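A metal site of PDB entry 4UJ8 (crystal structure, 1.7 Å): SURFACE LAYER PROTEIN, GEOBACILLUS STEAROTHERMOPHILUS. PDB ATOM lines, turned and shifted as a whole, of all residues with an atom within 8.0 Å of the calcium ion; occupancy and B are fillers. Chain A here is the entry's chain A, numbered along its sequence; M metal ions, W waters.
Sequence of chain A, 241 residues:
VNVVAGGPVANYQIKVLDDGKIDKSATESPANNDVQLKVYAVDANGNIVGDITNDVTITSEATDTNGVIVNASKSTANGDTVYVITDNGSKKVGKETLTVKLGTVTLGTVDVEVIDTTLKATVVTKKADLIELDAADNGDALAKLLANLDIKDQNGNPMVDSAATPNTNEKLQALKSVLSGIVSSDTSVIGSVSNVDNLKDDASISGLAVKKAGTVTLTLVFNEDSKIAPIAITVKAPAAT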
ATOM      1  N   SER A  60     -13.185 -15.732  34.953  1.00  0.00           N
ATOM      2  CA  SER A  60     -13.783 -14.668  34.167  1.00  0.00           C
ATOM      3  C   SER A  60     -14.518 -15.326  33.020  1.00  0.00           C
ATOM      4  O   SER A  60     -14.461 -16.550  32.880  1.00  0.00           O
ATOM      5  CB  SER A  60     -12.721 -13.695  33.666  1.00  0.00           C
ATOM      6  OG  SER A  60     -11.720 -14.401  32.942  1.00  0.00           O
ATOM      7  N   GLU A  61     -15.200 -14.543  32.185  1.00  0.00           N
ATOM      8  CA  GLU A  61     -15.988 -15.096  31.089  1.00  0.00           C
ATOM      9  C   GLU A  61     -15.135 -15.996  30.193  1.00  0.00           C
ATOM     10  O   GLU A  61     -14.003 -15.660  29.835  1.00  0.00           O
ATOM     11  CB  GLU A  61     -16.620 -13.980  30.261  1.00  0.00           C
ATOM     12  CG  GLU A  61     -15.615 -12.953  29.763  1.00  0.00           C
ATOM     13  CD  GLU A  61     -16.238 -11.940  28.836  1.00  0.00           C
ATOM     14  OE1 GLU A  61     -17.475 -11.867  28.761  1.00  0.00           O
ATOM     15  OE2 GLU A  61     -15.474 -11.195  28.178  1.00  0.00           O
ATOM     16  N   ALA A  62     -15.691 -17.166  29.871  1.00  0.00           N
ATOM     17  CA  ALA A  62     -14.992 -18.141  29.041  1.00  0.00           C
ATOM     18  C   ALA A  62     -14.656 -17.573  27.674  1.00  0.00           C
ATOM     19  O   ALA A  62     -13.506 -17.598  27.230  1.00  0.00           O
ATOM     20  CB  ALA A  62     -15.830 -19.408  28.899  1.00  0.00           C
ATOM     21  N   THR A  63     -15.667 -17.044  26.991  1.00  0.00           N
ATOM     22  CA  THR A  63     -15.475 -16.405  25.701  1.00  0.00           C
ATOM     23  C   THR A  63     -15.439 -14.889  25.902  1.00  0.00           C
ATOM     24  O   THR A  63     -16.319 -14.330  26.555  1.00  0.00           O
ATOM     25  CB  THR A  63     -16.578 -16.799  24.709  1.00  0.00           C
ATOM     26  OG1 THR A  63     -16.185 -17.993  24.030  1.00  0.00           O
ATOM     27  CG2 THR A  63     -16.814 -15.704  23.677  1.00  0.00           C
ATOM     28  N   ASP A  64     -14.411 -14.246  25.357  1.00  0.00           N
ATOM     29  CA  ASP A  64     -14.243 -12.812  25.511  1.00  0.00           C
ATOM     30  C   ASP A  64     -15.360 -12.045  24.811  1.00  0.00           C
ATOM     31  O   ASP A  64     -15.794 -12.427  23.734  1.00  0.00           O
ATOM     32  CB  ASP A  64     -12.897 -12.348  24.959  1.00  0.00           C
ATOM     33  CG  ASP A  64     -12.704 -10.847  25.086  1.00  0.00           C
ATOM     34  OD1 ASP A  64     -12.977 -10.316  26.182  1.00  0.00           O
ATOM     35  OD2 ASP A  64     -12.304 -10.209  24.098  1.00  0.00           O
ATOM     36  N   THR A  65     -15.812 -10.960  25.440  1.00  0.00           N
ATOM     37  CA  THR A  65     -16.887 -10.148  24.866  1.00  0.00           C
ATOM     38  C   THR A  65     -16.630  -8.643  24.974  1.00  0.00           C
ATOM     39  O   THR A  65     -17.504  -7.846  24.617  1.00  0.00           O
ATOM     40  CB  THR A  65     -18.247 -10.428  25.547  1.00  0.00           C
ATOM     41  OG1 THR A  65     -18.198 -10.016  26.920  1.00  0.00           O
ATOM     42  CG2 THR A  65     -18.606 -11.916  25.458  1.00  0.00           C
ATOM     43  N   ASN A  66     -15.461  -8.245  25.458  1.00  0.00           N
ATOM     44  CA  ASN A  66     -15.188  -6.819  25.649  1.00  0.00           C
ATOM     45  C   ASN A  66     -13.752  -6.382  25.353  1.00  0.00           C
ATOM     46  O   ASN A  66     -13.400  -5.229  25.606  1.00  0.00           O
ATOM     47  CB  ASN A  66     -15.567  -6.393  27.072  1.00  0.00           C
ATOM     48  CG  ASN A  66     -14.753  -7.108  28.137  1.00  0.00           C
ATOM     49  OD1 ASN A  66     -14.091  -8.115  27.861  1.00  0.00           O
ATOM     50  ND2 ASN A  66     -14.789  -6.593  29.355  1.00  0.00           N
ATOM     51  N   GLY A  67     -12.935  -7.286  24.833  1.00  0.00           N
ATOM     52  CA  GLY A  67     -11.547  -6.974  24.526  1.00  0.00           C
ATOM     53  C   GLY A  67     -10.674  -6.825  25.747  1.00  0.00           C
ATOM     54  O   GLY A  67      -9.547  -6.335  25.672  1.00  0.00           O
ATOM     55  N   VAL A  68     -11.208  -7.240  26.894  1.00  0.00           N
ATOM     56  CA  VAL A  68     -10.438  -7.241  28.133  1.00  0.00           C
ATOM     57  C   VAL A  68     -10.243  -8.679  28.607  1.00  0.00           C
ATOM     58  O   VAL A  68     -11.204  -9.385  28.920  1.00  0.00           O
ATOM     59  CB  VAL A  68     -11.117  -6.409  29.215  1.00  0.00           C
ATOM     60  CG1 VAL A  68     -10.248  -6.344  30.479  1.00  0.00           C
ATOM     61  CG2 VAL A  68     -11.398  -4.995  28.701  1.00  0.00           C
ATOM     62  N   ILE A  69      -8.999  -9.130  28.650  1.00  0.00           N
ATOM     63  CA  ILE A  69      -8.735 -10.527  28.983  1.00  0.00           C
ATOM     64  C   ILE A  69      -7.721 -10.579  30.105  1.00  0.00           C
ATOM     65  O   ILE A  69      -6.644  -9.989  30.011  1.00  0.00           O
ATOM     66  CB  ILE A  69      -8.227 -11.326  27.764  1.00  0.00           C
ATOM     67  CG1 ILE A  69      -9.155 -11.137  26.563  1.00  0.00           C
ATOM     68  CG2 ILE A  69      -8.110 -12.815  28.123  1.00  0.00           C
ATOM     69  CD1 ILE A  69      -8.664 -11.846  25.295  1.00  0.00           C
ATOM     70  N   VAL A  70      -8.084 -11.275  31.172  1.00  0.00           N
ATOM     71  CA  VAL A  70      -7.194 -11.384  32.319  1.00  0.00           C
ATOM     72  C   VAL A  70      -6.981 -12.837  32.744  1.00  0.00           C
ATOM     73  O   VAL A  70      -7.800 -13.713  32.487  1.00  0.00           O
ATOM     74  CB  VAL A  70      -7.713 -10.576  33.538  1.00  0.00           C
ATOM     75  CG1 VAL A  70      -7.859  -9.087  33.174  1.00  0.00           C
ATOM     76  CG2 VAL A  70      -9.035 -11.151  34.071  1.00  0.00           C
ATOM     77  N   SER A  90      -5.240  -8.213  26.523  1.00  0.00           N
ATOM     78  CA  SER A  90      -6.301  -7.235  26.359  1.00  0.00           C
ATOM     79  C   SER A  90      -6.013  -6.307  25.194  1.00  0.00           C
ATOM     80  O   SER A  90      -4.985  -5.630  25.154  1.00  0.00           O
ATOM     81  CB  SER A  90      -6.510  -6.404  27.623  1.00  0.00           C
ATOM     82  OG  SER A  90      -6.877  -7.214  28.731  1.00  0.00           O
ATOM     83  N   LYS A  95     -13.527  -2.717  32.328  1.00  0.00           N
ATOM     84  CA  LYS A  95     -13.781  -3.635  33.431  1.00  0.00           C
ATOM     85  C   LYS A  95     -14.031  -5.077  33.025  1.00  0.00           C
ATOM     86  O   LYS A  95     -14.625  -5.357  31.971  1.00  0.00           O
ATOM     87  CB  LYS A  95     -14.966  -3.137  34.259  1.00  0.00           C
ATOM     88  CG  LYS A  95     -14.629  -1.983  35.173  1.00  0.00           C
ATOM     89  CD  LYS A  95     -15.876  -1.420  35.837  1.00  0.00           C
ATOM     90  CE  LYS A  95     -15.545  -0.205  36.692  1.00  0.00           C
ATOM     91  NZ  LYS A  95     -16.752   0.294  37.428  1.00  0.00           N
ATOM     92  N   GLU A  96     -13.589  -5.989  33.883  1.00  0.00           N
ATOM     93  CA  GLU A  96     -13.765  -7.418  33.656  1.00  0.00           C
ATOM     94  C   GLU A  96     -14.250  -8.025  34.969  1.00  0.00           C
ATOM     95  O   GLU A  96     -13.669  -7.788  36.024  1.00  0.00           O
ATOM     96  CB  GLU A  96     -12.458  -8.066  33.175  1.00  0.00           C
ATOM     97  CG  GLU A  96     -12.552  -9.540  32.849  1.00  0.00           C
ATOM     98  CD  GLU A  96     -13.131  -9.824  31.471  1.00  0.00           C
ATOM     99  OE1 GLU A  96     -13.732  -8.915  30.854  1.00  0.00           O
ATOM    100  OE2 GLU A  96     -12.985 -10.975  30.989  1.00  0.00           O
ATOM    101  N   THR A  97     -15.335  -8.783  34.904  1.00  0.00           N
ATOM    102  CA  THR A  97     -15.966  -9.317  36.107  1.00  0.00           C
ATOM    103  C   THR A  97     -15.388 -10.665  36.496  1.00  0.00           C
ATOM    104  O   THR A  97     -15.407 -11.604  35.704  1.00  0.00           O
ATOM    105  CB  THR A  97     -17.492  -9.459  35.916  1.00  0.00           C
ATOM    106  OG1 THR A  97     -18.057  -8.172  35.622  1.00  0.00           O
ATOM    107  CG2 THR A  97     -18.141 -10.018  37.174  1.00  0.00           C
HETATM  108 CA    CA M   1     -13.362 -10.310  28.550  1.00  0.00          CA
HETATM  109  O   HOH W   1     -12.422 -12.518  28.301  1.00  0.00           O
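OE2 of Glu 61 binds the calcium ion, 2.3 Å away.
The calcium ion is bound by O of Val 68 (2.4 Å).
The side-chain carboxylate (OD1) of Asp 64 binds the calcium ion (2.4 Å).
The calcium ion is bound by water W1.
The side-chain amide oxygen (OD1) of Asn 66 is bound to the calcium ion, at 2.4 Å.
The side-chain carboxylate (OE2) of Glu 96 is bound to the calcium ion (2.6 Å).
The side-chain carboxylate (OE1) of Glu 96 binds the calcium ion (2.7 Å).
Five residues have an atom within 4 Å of the calcium ion: Glu 61, Asp 64, Asn 66, Val 68 and Glu 96.
The nearest printed residue that does not touch the calcium ion is Thr 65 (4.01 Å).
OE1 of Glu 61 sits at hydrogen-bond distance from OG1 of Thr 65 (2.7 Å).
The backbone NH (N) of Gly 67 is in hydrogen-bond range of the side-chain carboxylate (OD2) of Asp 64, at 3.1 Å.
ND2 of Asn 66 is in hydrogen-bond range of O of Lys 95 (2.9 Å).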
